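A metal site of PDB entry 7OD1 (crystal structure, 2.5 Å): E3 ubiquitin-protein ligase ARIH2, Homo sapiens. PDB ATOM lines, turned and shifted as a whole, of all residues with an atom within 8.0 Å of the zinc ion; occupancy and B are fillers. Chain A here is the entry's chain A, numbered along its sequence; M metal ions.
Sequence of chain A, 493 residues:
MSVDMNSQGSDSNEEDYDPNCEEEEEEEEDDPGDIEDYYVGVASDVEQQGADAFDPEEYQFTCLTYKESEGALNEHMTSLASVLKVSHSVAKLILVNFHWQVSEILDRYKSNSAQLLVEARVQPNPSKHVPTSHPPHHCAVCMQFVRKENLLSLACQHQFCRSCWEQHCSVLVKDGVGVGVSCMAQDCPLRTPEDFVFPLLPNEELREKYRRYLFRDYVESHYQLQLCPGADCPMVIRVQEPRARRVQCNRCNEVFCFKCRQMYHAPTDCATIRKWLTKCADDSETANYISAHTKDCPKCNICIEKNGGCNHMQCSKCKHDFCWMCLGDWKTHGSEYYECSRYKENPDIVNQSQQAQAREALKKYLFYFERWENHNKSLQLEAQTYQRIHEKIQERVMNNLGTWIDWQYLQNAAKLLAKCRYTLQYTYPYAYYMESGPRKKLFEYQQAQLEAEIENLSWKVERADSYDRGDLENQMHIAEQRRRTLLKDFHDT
OG1 of Thr 268 is in hydrogen-bond range of O of His 265 (2.6 Å). The backbone carbonyl oxygen (O) of Cys 260 lies close to the side-chain amide oxygen (OE1) of Gln 262 (3.3 Å). SG of Cys 257 sits close to N of Lys 259 (3.5 Å). The backbone NH (N) of Cys 257 lies within hydrogen-bond range of the backbone carbonyl oxygen (O) of Gln 262 (2.7 Å).
Four residues have an atom within 4 Å of the zinc ion: Cys 257, Cys 260, His 265 and Cys 270.
The zinc ion is bound by NE2 of His 265 (2.0 Å), SG of Cys 260 (2.3 Å), SG of Cys 257 (2.3 Å) and SG of Cys 270 (2.3 Å). The zinc ion has four donor atoms within binding distance.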
ATOM      1  N   ARG A 243     -12.014   6.903   4.853  1.00  0.00           N
ATOM      2  CA  ARG A 243     -12.932   7.947   4.412  1.00  0.00           C
ATOM      3  C   ARG A 243     -14.205   7.284   3.902  1.00  0.00           C
ATOM      4  O   ARG A 243     -14.307   6.066   3.829  1.00  0.00           O
ATOM      5  CB  ARG A 243     -12.312   8.836   3.330  1.00  0.00           C
ATOM      6  CG  ARG A 243     -10.860   9.209   3.562  1.00  0.00           C
ATOM      7  CD  ARG A 243     -10.736  10.562   4.247  1.00  0.00           C
ATOM      8  NE  ARG A 243      -9.453  10.760   4.919  1.00  0.00           N
ATOM      9  CZ  ARG A 243      -8.263  10.695   4.336  1.00  0.00           C
ATOM     10  NH1 ARG A 243      -8.126  10.493   3.042  1.00  0.00           N
ATOM     11  NH2 ARG A 243      -7.165  10.853   5.078  1.00  0.00           N
ATOM     12  N   ALA A 244     -15.190   8.119   3.539  1.00  0.00           N
ATOM     13  CA  ALA A 244     -16.428   7.628   2.943  1.00  0.00           C
ATOM     14  C   ALA A 244     -16.215   7.548   1.427  1.00  0.00           C
ATOM     15  O   ALA A 244     -16.562   8.452   0.664  1.00  0.00           O
ATOM     16  CB  ALA A 244     -17.595   8.528   3.299  1.00  0.00           C
ATOM     17  N   ARG A 245     -15.631   6.431   0.999  1.00  0.00           N
ATOM     18  CA  ARG A 245     -15.302   6.218  -0.408  1.00  0.00           C
ATOM     19  C   ARG A 245     -15.701   4.809  -0.803  1.00  0.00           C
ATOM     20  O   ARG A 245     -15.984   3.952   0.041  1.00  0.00           O
ATOM     21  CB  ARG A 245     -13.809   6.459  -0.671  1.00  0.00           C
ATOM     22  CG  ARG A 245     -13.323   7.850  -0.292  1.00  0.00           C
ATOM     23  CD  ARG A 245     -13.226   8.760  -1.500  1.00  0.00           C
ATOM     24  NE  ARG A 245     -13.199  10.172  -1.120  1.00  0.00           N
ATOM     25  CZ  ARG A 245     -12.137  10.796  -0.643  1.00  0.00           C
ATOM     26  NH1 ARG A 245     -10.980  10.168  -0.470  1.00  0.00           N
ATOM     27  NH2 ARG A 245     -12.226  12.081  -0.328  1.00  0.00           N
ATOM     28  N   PHE A 256     -19.457  -1.179  -1.738  1.00  0.00           N
ATOM     29  CA  PHE A 256     -20.026  -0.486  -0.589  1.00  0.00           C
ATOM     30  C   PHE A 256     -19.130   0.681  -0.188  1.00  0.00           C
ATOM     31  O   PHE A 256     -17.966   0.777  -0.585  1.00  0.00           O
ATOM     32  CB  PHE A 256     -20.244  -1.434   0.599  1.00  0.00           C
ATOM     33  CG  PHE A 256     -18.990  -2.088   1.112  1.00  0.00           C
ATOM     34  CD1 PHE A 256     -18.351  -3.090   0.377  1.00  0.00           C
ATOM     35  CD2 PHE A 256     -18.453  -1.720   2.330  1.00  0.00           C
ATOM     36  CE1 PHE A 256     -17.199  -3.688   0.846  1.00  0.00           C
ATOM     37  CE2 PHE A 256     -17.297  -2.325   2.817  1.00  0.00           C
ATOM     38  CZ  PHE A 256     -16.677  -3.308   2.072  1.00  0.00           C
ATOM     39  N   CYS A 257     -19.708   1.581   0.604  1.00  0.00           N
ATOM     40  CA  CYS A 257     -18.960   2.664   1.213  1.00  0.00           C
ATOM     41  C   CYS A 257     -18.164   2.135   2.398  1.00  0.00           C
ATOM     42  O   CYS A 257     -18.642   1.277   3.154  1.00  0.00           O
ATOM     43  CB  CYS A 257     -19.908   3.783   1.668  1.00  0.00           C
ATOM     44  SG  CYS A 257     -19.173   5.060   2.735  1.00  0.00           S
ATOM     45  N   PHE A 258     -16.943   2.639   2.566  1.00  0.00           N
ATOM     46  CA  PHE A 258     -16.072   2.112   3.604  1.00  0.00           C
ATOM     47  C   PHE A 258     -16.515   2.560   4.993  1.00  0.00           C
ATOM     48  O   PHE A 258     -16.436   1.796   5.955  1.00  0.00           O
ATOM     49  CB  PHE A 258     -14.626   2.511   3.356  1.00  0.00           C
ATOM     50  CG  PHE A 258     -13.655   1.922   4.337  1.00  0.00           C
ATOM     51  CD1 PHE A 258     -13.227   0.606   4.197  1.00  0.00           C
ATOM     52  CD2 PHE A 258     -13.180   2.664   5.403  1.00  0.00           C
ATOM     53  CE1 PHE A 258     -12.345   0.055   5.104  1.00  0.00           C
ATOM     54  CE2 PHE A 258     -12.299   2.113   6.310  1.00  0.00           C
ATOM     55  CZ  PHE A 258     -11.882   0.810   6.155  1.00  0.00           C
ATOM     56  N   LYS A 259     -16.980   3.804   5.115  1.00  0.00           N
ATOM     57  CA  LYS A 259     -17.276   4.351   6.432  1.00  0.00           C
ATOM     58  C   LYS A 259     -18.489   3.682   7.062  1.00  0.00           C
ATOM     59  O   LYS A 259     -18.415   3.161   8.181  1.00  0.00           O
ATOM     60  CB  LYS A 259     -17.472   5.866   6.355  1.00  0.00           C
ATOM     61  CG  LYS A 259     -17.441   6.564   7.711  1.00  0.00           C
ATOM     62  CD  LYS A 259     -16.987   8.005   7.603  1.00  0.00           C
ATOM     63  CE  LYS A 259     -17.475   8.835   8.785  1.00  0.00           C
ATOM     64  NZ  LYS A 259     -16.681  10.073   8.985  1.00  0.00           N
ATOM     65  N   CYS A 260     -19.622   3.679   6.364  1.00  0.00           N
ATOM     66  CA  CYS A 260     -20.866   3.202   6.964  1.00  0.00           C
ATOM     67  C   CYS A 260     -21.190   1.761   6.606  1.00  0.00           C
ATOM     68  O   CYS A 260     -22.122   1.194   7.179  1.00  0.00           O
ATOM     69  CB  CYS A 260     -22.050   4.075   6.528  1.00  0.00           C
ATOM     70  SG  CYS A 260     -22.296   4.224   4.752  1.00  0.00           S
ATOM     71  N   ARG A 261     -20.460   1.159   5.663  1.00  0.00           N
ATOM     72  CA  ARG A 261     -20.669  -0.213   5.185  1.00  0.00           C
ATOM     73  C   ARG A 261     -21.990  -0.380   4.446  1.00  0.00           C
ATOM     74  O   ARG A 261     -22.496  -1.506   4.322  1.00  0.00           O
ATOM     75  CB  ARG A 261     -20.588  -1.226   6.337  1.00  0.00           C
ATOM     76  CG  ARG A 261     -19.234  -1.888   6.497  1.00  0.00           C
ATOM     77  CD  ARG A 261     -19.229  -2.805   7.702  1.00  0.00           C
ATOM     78  NE  ARG A 261     -19.352  -4.203   7.326  1.00  0.00           N
ATOM     79  CZ  ARG A 261     -20.392  -4.972   7.619  1.00  0.00           C
ATOM     80  NH1 ARG A 261     -21.425  -4.500   8.297  1.00  0.00           N
ATOM     81  NH2 ARG A 261     -20.394  -6.247   7.241  1.00  0.00           N
ATOM     82  N   GLN A 262     -22.569   0.704   3.944  1.00  0.00           N
ATOM     83  CA  GLN A 262     -23.785   0.657   3.150  1.00  0.00           C
ATOM     84  C   GLN A 262     -23.440   0.895   1.679  1.00  0.00           C
ATOM     85  O   GLN A 262     -22.268   0.942   1.294  1.00  0.00           O
ATOM     86  CB  GLN A 262     -24.809   1.670   3.669  1.00  0.00           C
ATOM     87  CG  GLN A 262     -25.006   1.618   5.176  1.00  0.00           C
ATOM     88  CD  GLN A 262     -25.572   0.288   5.644  1.00  0.00           C
ATOM     89  OE1 GLN A 262     -24.994  -0.368   6.514  1.00  0.00           O
ATOM     90  NE2 GLN A 262     -26.701  -0.103   5.084  1.00  0.00           N
ATOM     91  N   MET A 263     -24.472   1.054   0.855  1.00  0.00           N
ATOM     92  CA  MET A 263     -24.273   1.302  -0.568  1.00  0.00           C
ATOM     93  C   MET A 263     -23.484   2.582  -0.789  1.00  0.00           C
ATOM     94  O   MET A 263     -23.631   3.558  -0.042  1.00  0.00           O
ATOM     95  CB  MET A 263     -25.615   1.378  -1.289  1.00  0.00           C
ATOM     96  CG  MET A 263     -25.986   0.120  -2.069  1.00  0.00           C
ATOM     97  SD  MET A 263     -27.376   0.375  -3.181  1.00  0.00           S
ATOM     98  CE  MET A 263     -28.433  -0.994  -2.738  1.00  0.00           C
ATOM     99  N   TYR A 264     -22.633   2.583  -1.817  1.00  0.00           N
ATOM    100  CA  TYR A 264     -21.870   3.763  -2.178  1.00  0.00           C
ATOM    101  C   TYR A 264     -22.820   4.926  -2.459  1.00  0.00           C
ATOM    102  O   TYR A 264     -23.799   4.769  -3.183  1.00  0.00           O
ATOM    103  CB  TYR A 264     -20.998   3.475  -3.396  1.00  0.00           C
ATOM    104  CG  TYR A 264     -20.157   4.635  -3.868  1.00  0.00           C
ATOM    105  CD1 TYR A 264     -19.410   5.389  -2.978  1.00  0.00           C
ATOM    106  CD2 TYR A 264     -20.101   4.967  -5.218  1.00  0.00           C
ATOM    107  CE1 TYR A 264     -18.638   6.455  -3.416  1.00  0.00           C
ATOM    108  CE2 TYR A 264     -19.336   6.029  -5.667  1.00  0.00           C
ATOM    109  CZ  TYR A 264     -18.606   6.766  -4.758  1.00  0.00           C
ATOM    110  OH  TYR A 264     -17.840   7.825  -5.197  1.00  0.00           O
ATOM    111  N   HIS A 265     -22.527   6.086  -1.872  1.00  0.00           N
ATOM    112  CA  HIS A 265     -23.501   7.166  -1.808  1.00  0.00           C
ATOM    113  C   HIS A 265     -22.858   8.532  -1.964  1.00  0.00           C
ATOM    114  O   HIS A 265     -23.265   9.513  -1.332  1.00  0.00           O
ATOM    115  CB  HIS A 265     -24.289   7.112  -0.497  1.00  0.00           C
ATOM    116  CG  HIS A 265     -23.419   7.153   0.721  1.00  0.00           C
ATOM    117  ND1 HIS A 265     -22.785   8.302   1.140  1.00  0.00           N
ATOM    118  CD2 HIS A 265     -23.073   6.188   1.602  1.00  0.00           C
ATOM    119  CE1 HIS A 265     -22.086   8.047   2.231  1.00  0.00           C
ATOM    120  NE2 HIS A 265     -22.246   6.772   2.531  1.00  0.00           N
ATOM    121  N   ALA A 266     -21.846   8.642  -2.813  1.00  0.00           N
ATOM    122  CA  ALA A 266     -21.283   9.960  -3.056  1.00  0.00           C
ATOM    123  C   ALA A 266     -22.193  10.764  -3.971  1.00  0.00           C
ATOM    124  O   ALA A 266     -22.848  10.197  -4.855  1.00  0.00           O
ATOM    125  CB  ALA A 266     -19.890   9.845  -3.670  1.00  0.00           C
ATOM    126  N   THR A 268     -23.193  12.526  -1.170  1.00  0.00           N
ATOM    127  CA  THR A 268     -23.743  12.632   0.181  1.00  0.00           C
ATOM    128  C   THR A 268     -22.844  11.915   1.185  1.00  0.00           C
ATOM    129  O   THR A 268     -22.142  10.958   0.856  1.00  0.00           O
ATOM    130  CB  THR A 268     -25.149  12.033   0.247  1.00  0.00           C
ATOM    131  OG1 THR A 268     -25.066  10.612   0.123  1.00  0.00           O
ATOM    132  CG2 THR A 268     -26.016  12.583  -0.870  1.00  0.00           C
ATOM    133  N   ASP A 269     -22.861  12.396   2.426  1.00  0.00           N
ATOM    134  CA  ASP A 269     -22.171  11.700   3.496  1.00  0.00           C
ATOM    135  C   ASP A 269     -23.079  10.595   4.048  1.00  0.00           C
ATOM    136  O   ASP A 269     -24.215  10.415   3.611  1.00  0.00           O
ATOM    137  CB  ASP A 269     -21.691  12.675   4.571  1.00  0.00           C
ATOM    138  CG  ASP A 269     -22.836  13.415   5.266  1.00  0.00           C
ATOM    139  OD1 ASP A 269     -23.925  12.855   5.441  1.00  0.00           O
ATOM    140  OD2 ASP A 269     -22.608  14.587   5.654  1.00  0.00           O
ATOM    141  N   CYS A 270     -22.578   9.851   5.032  1.00  0.00           N
ATOM    142  CA  CYS A 270     -23.273   8.650   5.479  1.00  0.00           C
ATOM    143  C   CYS A 270     -24.558   8.993   6.231  1.00  0.00           C
ATOM    144  O   CYS A 270     -25.603   8.380   5.983  1.00  0.00           O
ATOM    145  CB  CYS A 270     -22.331   7.802   6.338  1.00  0.00           C
ATOM    146  SG  CYS A 270     -20.703   7.473   5.569  1.00  0.00           S
ATOM    147  N   ALA A 271     -24.503   9.966   7.139  1.00  0.00           N
ATOM    148  CA  ALA A 271     -25.684  10.321   7.916  1.00  0.00           C
ATOM    149  C   ALA A 271     -26.798  10.855   7.033  1.00  0.00           C
ATOM    150  O   ALA A 271     -27.973  10.526   7.225  1.00  0.00           O
ATOM    151  CB  ALA A 271     -25.312  11.349   8.992  1.00  0.00           C
ATOM    152  N   ILE A 273     -27.424  10.274   3.825  1.00  0.00           N
ATOM    153  CA  ILE A 273     -28.068   9.245   3.016  1.00  0.00           C
ATOM    154  C   ILE A 273     -28.870   8.297   3.887  1.00  0.00           C
ATOM    155  O   ILE A 273     -29.916   7.785   3.459  1.00  0.00           O
ATOM    156  CB  ILE A 273     -27.032   8.498   2.147  1.00  0.00           C
ATOM    157  CG1 ILE A 273     -27.731   7.443   1.297  1.00  0.00           C
ATOM    158  CG2 ILE A 273     -25.979   7.836   2.996  1.00  0.00           C
ATOM    159  CD1 ILE A 273     -28.314   7.992   0.018  1.00  0.00           C
ATOM    160  N   ARG A 274     -28.427   8.038   5.120  1.00  0.00           N
ATOM    161  CA  ARG A 274     -29.249   7.234   6.027  1.00  0.00           C
ATOM    162  C   ARG A 274     -30.583   7.921   6.297  1.00  0.00           C
ATOM    163  O   ARG A 274     -31.655   7.298   6.226  1.00  0.00           O
ATOM    164  CB  ARG A 274     -28.503   6.967   7.332  1.00  0.00           C
ATOM    165  CG  ARG A 274     -29.251   6.004   8.250  1.00  0.00           C
ATOM    166  CD  ARG A 274     -29.011   6.315   9.720  1.00  0.00           C
ATOM    167  NE  ARG A 274     -27.656   6.793   9.979  1.00  0.00           N
ATOM    168  CZ  ARG A 274     -27.364   8.035  10.335  1.00  0.00           C
ATOM    169  NH1 ARG A 274     -28.296   8.960  10.474  1.00  0.00           N
ATOM    170  NH2 ARG A 274     -26.089   8.362  10.556  1.00  0.00           N
ATOM    171  N   HIS A 491     -17.688  16.167  -3.006  1.00  0.00           N
ATOM    172  CA  HIS A 491     -17.428  14.939  -2.247  1.00  0.00           C
ATOM    173  C   HIS A 491     -16.406  15.287  -1.166  1.00  0.00           C
ATOM    174  O   HIS A 491     -15.198  15.160  -1.352  1.00  0.00           O
ATOM    175  CB  HIS A 491     -16.926  13.818  -3.148  1.00  0.00           C
ATOM    176  CG  HIS A 491     -16.841  12.490  -2.475  1.00  0.00           C
ATOM    177  ND1 HIS A 491     -17.338  12.260  -1.208  1.00  0.00           N
ATOM    178  CD2 HIS A 491     -16.313  11.312  -2.891  1.00  0.00           C
ATOM    179  CE1 HIS A 491     -17.117  10.995  -0.868  1.00  0.00           C
ATOM    180  NE2 HIS A 491     -16.493  10.401  -1.872  1.00  0.00           N
HETATM  181 ZN    ZN M   1     -20.993   5.912   3.883  1.00  0.00          ZN
